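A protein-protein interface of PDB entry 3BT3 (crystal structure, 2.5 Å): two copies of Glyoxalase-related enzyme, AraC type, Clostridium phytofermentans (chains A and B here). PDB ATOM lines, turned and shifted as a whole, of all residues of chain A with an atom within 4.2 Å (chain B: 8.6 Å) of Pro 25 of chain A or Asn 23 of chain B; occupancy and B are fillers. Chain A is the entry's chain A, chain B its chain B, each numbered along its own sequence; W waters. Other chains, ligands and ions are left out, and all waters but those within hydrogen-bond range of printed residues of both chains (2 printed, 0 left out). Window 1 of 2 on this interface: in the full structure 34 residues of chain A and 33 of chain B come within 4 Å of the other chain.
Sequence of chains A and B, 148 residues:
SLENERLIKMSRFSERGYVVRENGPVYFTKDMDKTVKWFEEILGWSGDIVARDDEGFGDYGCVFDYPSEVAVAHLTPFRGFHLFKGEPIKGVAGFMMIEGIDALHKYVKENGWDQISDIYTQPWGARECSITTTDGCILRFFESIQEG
The backbone carbonyl oxygen (O) of Gly 24 of chain A is in hydrogen-bond range of a ring nitrogen (ND1) of His 82 of chain A, at 3.3 Å.
The backbone NH (N) of His 82 of chain A lies within hydrogen-bond range of the backbone carbonyl oxygen (O) of Pro 25 of chain A.
N of His 82 of chain B lies within hydrogen-bond range of O of Pro 25 of chain B (3.0 Å).
Of chain A, only Pro 25 (3.2 Å), Arg 79 (2.9 Å), Gly 80 (3.4 Å), Phe 81 (3.8 Å) and Met 96 (3.6 Å) come within 4 Å of Asn 23 of chain B.
Gly 24 of chain A touches just one residue of chain B: Phe 95.
Of chain B, only Val 92, Ala 93 and Phe 95 come within 4 Å of Val 26 of chain A.
Of chain B, only Asn 23 comes within 4 Å of Gly 80 of chain A.
Of the printed residues of chain B, Arg 79 of chain A touches Arg 21 and Asn 23.
Of the printed residues of chain A, Gly 80 of chain B touches Asn 23 (3.7 Å).
Of the printed residues of chain B, Met 96 of chain A touches Glu 22 (3.0 Å) and Asn 23 (3.6 Å).
Printed residues of chain A within 4 Å of Val 92 of chain B: Val 26.
Pro 77 of chain B touches none of the printed residues of chain A.
Val 20 of chain B touches none of the printed residues of chain A.
The nearest residue of chain B that does not touch Pro 25 of chain A is Gly 24 of chain B (4.7 Å).
The nearest printed residue of chain A that does not touch Asn 23 of chain B is Asn 23 of chain A (4.9 Å).
The nearest printed residue of chain A that does not touch Gly 80 of chain B is Pro 25 of chain A (7.4 Å).
Water W1 lies within hydrogen-bond range of the backbone carbonyl oxygen of Phe 95 of chain B, the backbone NH of Gly 24 of chain A and the backbone NH of Asn 23 of chain A.
Water W2 lies within hydrogen-bond range of N of Phe 95 of chain B, O of Gly 24 of chain A and OD1 of Asn 23 of chain A.
ND2 of Asn 23 of chain A touches CG of Pro 25 of chain B, at 3.2 Å.
Asn 23 of chain A touches Gly 80 of chain B.
Pro 25 of chain A touches Asn 23 of chain B (CD to O, 3.2 Å).
Pro 25 of chain B touches Pro 25 of chain A.
Val 26 of chain A touches Val 92 of chain B.
O of Ala 93 of chain B touches CG2 of Val 26 of chain A (3.9 Å).
Phe 95 of chain B touches Val 26 of chain A.
CZ of Phe 81 of chain A touches OD1 of Asn 23 of chain B, at 3.8 Å.
His 82 of chain A touches Phe 95 of chain B.
Met 96 of chain A touches Glu 22 of chain B (CB to O, 3.0 Å).
ND2 of Asn 23 of chain A is in hydrogen-bond range of O of Arg 79 of chain B (3.1 Å).
The side-chain amide oxygen of Asn 23 of chain A sits close to the side-chain sulfur of Met 96 of chain B (3.7 Å).
NH2 of Arg 79 of chain A sits at hydrogen-bond distance from O of Arg 21 of chain B (3.5 Å).
ND2 of Asn 23 of chain B is in hydrogen-bond range of O of Arg 79 of chain A, 2.9 Å away.
O of Gly 80 of chain A lies within hydrogen-bond range of ND2 of Asn 23 of chain B (3.4 Å).
The side-chain sulfur (SD) of Met 96 of chain A lies close to the side-chain amide oxygen (OD1) of Asn 23 of chain B (3.7 Å).
Asn 23 of chain A touches Gly 80 of chain B, and with the chains exchanged Gly 80 of chain A touches Asn 23 of chain B.
Asn 23 of chain A touches Met 96 of chain B, and with the chains exchanged Met 96 of chain A touches Asn 23 of chain B.
Pro 25 of chain B touches its own counterpart, Pro 25 of chain A.
Phe 81 of chain A touches Asn 23 of chain B, but with the chains exchanged Asn 23 of chain A does not touch Phe 81 of chain B (4.2 Å).
Of the 17 pairs that touch across the chains among the printed residues, 9 have their exchanged pair printed and touching as well.
Of the 18 printed residues of chain B, 10 touch a printed residue of chain A.
Hydrophobic or aromatic side chains of chain B that line the printed part of chain A: Pro 25, Phe 95 and Met 96.
Hydrophobic or aromatic side chains of chain A within 4 Å of the printed part of chain B: Pro 25, Val 26, Phe 81, His 82 and Met 96.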
ATOM      1  N   ASN A  23       6.379  12.316   0.162  1.00  0.00           N
ATOM      2  CA  ASN A  23       7.516  11.472   0.466  1.00  0.00           C
ATOM      3  C   ASN A  23       7.203  10.469   1.553  1.00  0.00           C
ATOM      4  O   ASN A  23       7.739  10.556   2.645  1.00  0.00           O
ATOM      5  CB  ASN A  23       8.720  12.320   0.886  1.00  0.00           C
ATOM      6  CG  ASN A  23       9.959  11.484   1.118  1.00  0.00           C
ATOM      7  OD1 ASN A  23      10.224  10.540   0.378  1.00  0.00           O
ATOM      8  ND2 ASN A  23      10.732  11.831   2.136  1.00  0.00           N
ATOM      9  N   GLY A  24       6.329   9.516   1.249  1.00  0.00           N
ATOM     10  CA  GLY A  24       5.980   8.500   2.222  1.00  0.00           C
ATOM     11  C   GLY A  24       7.043   7.419   2.260  1.00  0.00           C
ATOM     12  O   GLY A  24       7.627   7.096   1.230  1.00  0.00           O
ATOM     13  N   PRO A  25       7.330   6.846   3.435  1.00  0.00           N
ATOM     14  CA  PRO A  25       8.341   5.793   3.571  1.00  0.00           C
ATOM     15  C   PRO A  25       8.032   4.536   2.761  1.00  0.00           C
ATOM     16  O   PRO A  25       6.870   4.259   2.451  1.00  0.00           O
ATOM     17  CB  PRO A  25       8.361   5.520   5.076  1.00  0.00           C
ATOM     18  CG  PRO A  25       7.004   5.944   5.536  1.00  0.00           C
ATOM     19  CD  PRO A  25       6.759   7.200   4.745  1.00  0.00           C
ATOM     20  N   VAL A  26       9.079   3.792   2.405  1.00  0.00           N
ATOM     21  CA  VAL A  26       8.920   2.558   1.643  1.00  0.00           C
ATOM     22  C   VAL A  26       8.957   1.337   2.555  1.00  0.00           C
ATOM     23  O   VAL A  26       9.602   1.352   3.602  1.00  0.00           O
ATOM     24  CB  VAL A  26      10.014   2.397   0.586  1.00  0.00           C
ATOM     25  CG1 VAL A  26       9.863   3.482  -0.466  1.00  0.00           C
ATOM     26  CG2 VAL A  26      11.397   2.434   1.249  1.00  0.00           C
ATOM     27  N   ARG A  79       0.997  10.095   3.933  1.00  0.00           N
ATOM     28  CA  ARG A  79       1.958   9.867   5.002  1.00  0.00           C
ATOM     29  C   ARG A  79       1.962   8.428   5.518  1.00  0.00           C
ATOM     30  O   ARG A  79       2.304   8.181   6.669  1.00  0.00           O
ATOM     31  CB  ARG A  79       1.695  10.821   6.170  1.00  0.00           C
ATOM     32  CG  ARG A  79       0.403  10.556   6.912  1.00  0.00           C
ATOM     33  CD  ARG A  79       0.527  11.066   8.332  1.00  0.00           C
ATOM     34  NE  ARG A  79       0.922  12.468   8.354  1.00  0.00           N
ATOM     35  CZ  ARG A  79       0.075  13.482   8.505  1.00  0.00           C
ATOM     36  NH1 ARG A  79      -1.225  13.251   8.656  1.00  0.00           N
ATOM     37  NH2 ARG A  79       0.528  14.729   8.490  1.00  0.00           N
ATOM     38  N   GLY A  80       1.572   7.481   4.672  1.00  0.00           N
ATOM     39  CA  GLY A  80       1.580   6.091   5.091  1.00  0.00           C
ATOM     40  C   GLY A  80       2.821   5.401   4.551  1.00  0.00           C
ATOM     41  O   GLY A  80       3.856   6.041   4.359  1.00  0.00           O
ATOM     42  N   PHE A  81       2.730   4.097   4.319  1.00  0.00           N
ATOM     43  CA  PHE A  81       3.852   3.344   3.760  1.00  0.00           C
ATOM     44  C   PHE A  81       3.502   2.874   2.356  1.00  0.00           C
ATOM     45  O   PHE A  81       2.369   2.467   2.096  1.00  0.00           O
ATOM     46  CB  PHE A  81       4.159   2.106   4.608  1.00  0.00           C
ATOM     47  CG  PHE A  81       4.837   2.404   5.912  1.00  0.00           C
ATOM     48  CD1 PHE A  81       6.220   2.559   5.975  1.00  0.00           C
ATOM     49  CD2 PHE A  81       4.093   2.527   7.083  1.00  0.00           C
ATOM     50  CE1 PHE A  81       6.855   2.834   7.188  1.00  0.00           C
ATOM     51  CE2 PHE A  81       4.715   2.804   8.301  1.00  0.00           C
ATOM     52  CZ  PHE A  81       6.099   2.956   8.354  1.00  0.00           C
ATOM     53  N   HIS A  82       4.462   2.958   1.443  1.00  0.00           N
ATOM     54  CA  HIS A  82       4.259   2.458   0.090  1.00  0.00           C
ATOM     55  C   HIS A  82       4.703   1.010   0.238  1.00  0.00           C
ATOM     56  O   HIS A  82       5.724   0.753   0.864  1.00  0.00           O
ATOM     57  CB  HIS A  82       5.180   3.146  -0.916  1.00  0.00           C
ATOM     58  CG  HIS A  82       4.786   4.550  -1.245  1.00  0.00           C
ATOM     59  ND1 HIS A  82       5.478   5.648  -0.779  1.00  0.00           N
ATOM     60  CD2 HIS A  82       3.776   5.034  -2.008  1.00  0.00           C
ATOM     61  CE1 HIS A  82       4.910   6.749  -1.240  1.00  0.00           C
ATOM     62  NE2 HIS A  82       3.877   6.403  -1.989  1.00  0.00           N
ATOM     63  N   MET A  96       7.941   7.013  13.579  1.00  0.00           N
ATOM     64  CA  MET A  96       6.867   7.990  13.568  1.00  0.00           C
ATOM     65  C   MET A  96       6.403   8.582  14.894  1.00  0.00           C
ATOM     66  O   MET A  96       6.290   7.897  15.907  1.00  0.00           O
ATOM     67  CB  MET A  96       5.673   7.432  12.763  1.00  0.00           C
ATOM     68  CG  MET A  96       5.086   6.086  13.197  1.00  0.00           C
ATOM     69  SD  MET A  96       3.930   5.343  11.933  1.00  0.00           S
ATOM     70  CE  MET A  96       4.896   4.031  11.395  1.00  0.00           C
ATOM     71  N   VAL B  20      -1.374   9.360  14.022  1.00  0.00           N
ATOM     72  CA  VAL B  20      -0.014   9.560  13.556  1.00  0.00           C
ATOM     73  C   VAL B  20       0.176  11.036  13.219  1.00  0.00           C
ATOM     74  O   VAL B  20      -0.574  11.587  12.421  1.00  0.00           O
ATOM     75  CB  VAL B  20       0.267   8.713  12.296  1.00  0.00           C
ATOM     76  CG1 VAL B  20       1.609   9.105  11.690  1.00  0.00           C
ATOM     77  CG2 VAL B  20       0.269   7.250  12.654  1.00  0.00           C
ATOM     78  N   ARG B  21       1.165  11.680  13.834  1.00  0.00           N
ATOM     79  CA  ARG B  21       1.408  13.095  13.561  1.00  0.00           C
ATOM     80  C   ARG B  21       2.387  13.240  12.407  1.00  0.00           C
ATOM     81  O   ARG B  21       2.173  14.033  11.496  1.00  0.00           O
ATOM     82  CB  ARG B  21       1.969  13.813  14.794  1.00  0.00           C
ATOM     83  CG  ARG B  21       1.065  13.782  16.015  1.00  0.00           C
ATOM     84  CD  ARG B  21       0.749  15.197  16.511  1.00  0.00           C
ATOM     85  NE  ARG B  21      -0.162  15.884  15.603  1.00  0.00           N
ATOM     86  CZ  ARG B  21      -1.388  15.456  15.326  1.00  0.00           C
ATOM     87  NH1 ARG B  21      -1.845  14.347  15.894  1.00  0.00           N
ATOM     88  NH2 ARG B  21      -2.159  16.123  14.476  1.00  0.00           N
ATOM     89  N   GLU B  22       3.465  12.464  12.451  1.00  0.00           N
ATOM     90  CA  GLU B  22       4.477  12.505  11.412  1.00  0.00           C
ATOM     91  C   GLU B  22       4.998  11.112  11.138  1.00  0.00           C
ATOM     92  O   GLU B  22       5.098  10.286  12.052  1.00  0.00           O
ATOM     93  CB  GLU B  22       5.638  13.403  11.836  1.00  0.00           C
ATOM     94  CG  GLU B  22       5.392  14.874  11.600  1.00  0.00           C
ATOM     95  CD  GLU B  22       6.197  15.755  12.530  1.00  0.00           C
ATOM     96  OE1 GLU B  22       7.426  15.536  12.670  1.00  0.00           O
ATOM     97  OE2 GLU B  22       5.589  16.674  13.119  1.00  0.00           O
ATOM     98  N   ASN B  23       5.328  10.855   9.875  1.00  0.00           N
ATOM     99  CA  ASN B  23       5.856   9.565   9.484  1.00  0.00           C
ATOM    100  C   ASN B  23       6.859   9.710   8.350  1.00  0.00           C
ATOM    101  O   ASN B  23       6.648   9.206   7.252  1.00  0.00           O
ATOM    102  CB  ASN B  23       4.715   8.620   9.090  1.00  0.00           C
ATOM    103  CG  ASN B  23       5.206   7.229   8.691  1.00  0.00           C
ATOM    104  OD1 ASN B  23       6.109   6.673   9.309  1.00  0.00           O
ATOM    105  ND2 ASN B  23       4.591   6.658   7.665  1.00  0.00           N
ATOM    106  N   GLY B  24       7.961  10.402   8.631  1.00  0.00           N
ATOM    107  CA  GLY B  24       8.998  10.583   7.633  1.00  0.00           C
ATOM    108  C   GLY B  24       9.901   9.363   7.461  1.00  0.00           C
ATOM    109  O   GLY B  24      10.197   8.670   8.438  1.00  0.00           O
ATOM    110  N   PRO B  25      10.362   9.076   6.229  1.00  0.00           N
ATOM    111  CA  PRO B  25      11.235   7.931   5.940  1.00  0.00           C
ATOM    112  C   PRO B  25      12.547   7.956   6.706  1.00  0.00           C
ATOM    113  O   PRO B  25      13.050   9.018   7.075  1.00  0.00           O
ATOM    114  CB  PRO B  25      11.468   8.047   4.441  1.00  0.00           C
ATOM    115  CG  PRO B  25      11.461   9.533   4.237  1.00  0.00           C
ATOM    116  CD  PRO B  25      10.232   9.935   5.040  1.00  0.00           C
ATOM    117  N   VAL B  26      13.101   6.769   6.915  1.00  0.00           N
ATOM    118  CA  VAL B  26      14.358   6.597   7.624  1.00  0.00           C
ATOM    119  C   VAL B  26      15.494   6.379   6.627  1.00  0.00           C
ATOM    120  O   VAL B  26      15.283   5.880   5.517  1.00  0.00           O
ATOM    121  CB  VAL B  26      14.294   5.380   8.555  1.00  0.00           C
ATOM    122  CG1 VAL B  26      13.282   5.626   9.652  1.00  0.00           C
ATOM    123  CG2 VAL B  26      13.911   4.133   7.748  1.00  0.00           C
ATOM    124  N   PRO B  77       4.842  19.969   9.862  1.00  0.00           N
ATOM    125  CA  PRO B  77       4.892  18.728   9.084  1.00  0.00           C
ATOM    126  C   PRO B  77       6.344  18.325   8.833  1.00  0.00           C
ATOM    127  O   PRO B  77       7.258  19.125   9.063  1.00  0.00           O
ATOM    128  CB  PRO B  77       4.178  19.118   7.800  1.00  0.00           C
ATOM    129  CG  PRO B  77       4.683  20.528   7.591  1.00  0.00           C
ATOM    130  CD  PRO B  77       4.554  21.124   8.988  1.00  0.00           C
ATOM    131  N   PHE B  78       6.562  17.098   8.367  1.00  0.00           N
ATOM    132  CA  PHE B  78       7.919  16.634   8.079  1.00  0.00           C
ATOM    133  C   PHE B  78       7.966  15.647   6.912  1.00  0.00           C
ATOM    134  O   PHE B  78       7.496  14.517   7.027  1.00  0.00           O
ATOM    135  CB  PHE B  78       8.548  15.992   9.319  1.00  0.00           C
ATOM    136  CG  PHE B  78       9.975  15.562   9.114  1.00  0.00           C
ATOM    137  CD1 PHE B  78      10.969  16.503   8.855  1.00  0.00           C
ATOM    138  CD2 PHE B  78      10.317  14.213   9.123  1.00  0.00           C
ATOM    139  CE1 PHE B  78      12.283  16.108   8.600  1.00  0.00           C
ATOM    140  CE2 PHE B  78      11.630  13.803   8.869  1.00  0.00           C
ATOM    141  CZ  PHE B  78      12.615  14.751   8.606  1.00  0.00           C
ATOM    142  N   ARG B  79       8.544  16.081   5.793  1.00  0.00           N
ATOM    143  CA  ARG B  79       8.650  15.248   4.597  1.00  0.00           C
ATOM    144  C   ARG B  79      10.094  14.967   4.185  1.00  0.00           C
ATOM    145  O   ARG B  79      10.377  14.804   3.000  1.00  0.00           O
ATOM    146  CB  ARG B  79       7.959  15.926   3.418  1.00  0.00           C
ATOM    147  CG  ARG B  79       6.537  16.371   3.661  1.00  0.00           C
ATOM    148  CD  ARG B  79       6.050  17.136   2.446  1.00  0.00           C
ATOM    149  NE  ARG B  79       7.127  17.962   1.903  1.00  0.00           N
ATOM    150  CZ  ARG B  79       6.953  18.950   1.030  1.00  0.00           C
ATOM    151  NH1 ARG B  79       5.733  19.247   0.595  1.00  0.00           N
ATOM    152  NH2 ARG B  79       8.001  19.638   0.588  1.00  0.00           N
ATOM    153  N   GLY B  80      11.008  14.922   5.147  1.00  0.00           N
ATOM    154  CA  GLY B  80      12.394  14.664   4.807  1.00  0.00           C
ATOM    155  C   GLY B  80      12.826  13.295   5.279  1.00  0.00           C
ATOM    156  O   GLY B  80      11.999  12.425   5.521  1.00  0.00           O
ATOM    157  N   PHE B  81      14.127  13.094   5.407  1.00  0.00           N
ATOM    158  CA  PHE B  81      14.633  11.824   5.880  1.00  0.00           C
ATOM    159  C   PHE B  81      15.234  11.973   7.272  1.00  0.00           C
ATOM    160  O   PHE B  81      15.895  12.966   7.563  1.00  0.00           O
ATOM    161  CB  PHE B  81      15.729  11.305   4.952  1.00  0.00           C
ATOM    162  CG  PHE B  81      15.236  10.792   3.633  1.00  0.00           C
ATOM    163  CD1 PHE B  81      14.902   9.454   3.476  1.00  0.00           C
ATOM    164  CD2 PHE B  81      15.157  11.637   2.530  1.00  0.00           C
ATOM    165  CE1 PHE B  81      14.505   8.958   2.238  1.00  0.00           C
ATOM    166  CE2 PHE B  81      14.761  11.154   1.293  1.00  0.00           C
ATOM    167  CZ  PHE B  81      14.436   9.809   1.145  1.00  0.00           C
ATOM    168  N   HIS B  82      14.981  10.991   8.136  1.00  0.00           N
ATOM    169  CA  HIS B  82      15.589  10.972   9.466  1.00  0.00           C
ATOM    170  C   HIS B  82      16.908  10.273   9.176  1.00  0.00           C
ATOM    171  O   HIS B  82      16.950   9.347   8.370  1.00  0.00           O
ATOM    172  CB  HIS B  82      14.798  10.118  10.461  1.00  0.00           C
ATOM    173  CG  HIS B  82      13.511  10.732  10.900  1.00  0.00           C
ATOM    174  ND1 HIS B  82      12.282  10.265  10.484  1.00  0.00           N
ATOM    175  CD2 HIS B  82      13.259  11.789  11.706  1.00  0.00           C
ATOM    176  CE1 HIS B  82      11.328  11.009  11.015  1.00  0.00           C
ATOM    177  NE2 HIS B  82      11.895  11.940  11.760  1.00  0.00           N
ATOM    178  N   VAL B  92      16.313   0.419  -2.801  1.00  0.00           N
ATOM    179  CA  VAL B  92      15.479   1.609  -2.774  1.00  0.00           C
ATOM    180  C   VAL B  92      15.261   2.140  -1.357  1.00  0.00           C
ATOM    181  O   VAL B  92      14.794   1.412  -0.485  1.00  0.00           O
ATOM    182  CB  VAL B  92      14.106   1.311  -3.412  1.00  0.00           C
ATOM    183  CG1 VAL B  92      13.153   2.463  -3.171  1.00  0.00           C
ATOM    184  CG2 VAL B  92      14.274   1.047  -4.904  1.00  0.00           C
ATOM    185  N   ALA B  93      15.590   3.411  -1.138  1.00  0.00           N
ATOM    186  CA  ALA B  93      15.417   4.046   0.168  1.00  0.00           C
ATOM    187  C   ALA B  93      14.315   5.103   0.143  1.00  0.00           C
ATOM    188  O   ALA B  93      13.815   5.503   1.190  1.00  0.00           O
ATOM    189  CB  ALA B  93      16.723   4.680   0.617  1.00  0.00           C
ATOM    190  N   GLY B  94      13.944   5.560  -1.050  1.00  0.00           N
ATOM    191  CA  GLY B  94      12.902   6.565  -1.157  1.00  0.00           C
ATOM    192  C   GLY B  94      12.075   6.507  -2.433  1.00  0.00           C
ATOM    193  O   GLY B  94      12.561   6.107  -3.491  1.00  0.00           O
ATOM    194  N   PHE B  95      10.819   6.929  -2.314  1.00  0.00           N
ATOM    195  CA  PHE B  95       9.859   6.959  -3.411  1.00  0.00           C
ATOM    196  C   PHE B  95       9.104   8.270  -3.238  1.00  0.00           C
ATOM    197  O   PHE B  95       8.139   8.337  -2.469  1.00  0.00           O
ATOM    198  CB  PHE B  95       8.896   5.783  -3.278  1.00  0.00           C
ATOM    199  CG  PHE B  95       7.932   5.640  -4.429  1.00  0.00           C
ATOM    200  CD1 PHE B  95       8.393   5.404  -5.717  1.00  0.00           C
ATOM    201  CD2 PHE B  95       6.560   5.673  -4.207  1.00  0.00           C
ATOM    202  CE1 PHE B  95       7.504   5.194  -6.775  1.00  0.00           C
ATOM    203  CE2 PHE B  95       5.661   5.464  -5.255  1.00  0.00           C
ATOM    204  CZ  PHE B  95       6.137   5.223  -6.544  1.00  0.00           C
ATOM    205  N   MET B  96       9.545   9.300  -3.960  1.00  0.00           N
ATOM    206  CA  MET B  96       8.977  10.647  -3.871  1.00  0.00           C
ATOM    207  C   MET B  96       8.226  11.183  -5.087  1.00  0.00           C
ATOM    208  O   MET B  96       8.702  11.088  -6.222  1.00  0.00           O
ATOM    209  CB  MET B  96      10.092  11.659  -3.561  1.00  0.00           C
ATOM    210  CG  MET B  96      10.737  11.543  -2.199  1.00  0.00           C
ATOM    211  SD  MET B  96      12.148  12.688  -2.017  1.00  0.00           S
ATOM    212  CE  MET B  96      13.443  11.560  -2.157  1.00  0.00           C
HETATM  213  O   HOH W   1       6.031   9.453  -1.500  1.00  0.00           O
HETATM  214  O   HOH W   2      10.158   7.641   0.080  1.00  0.00           O
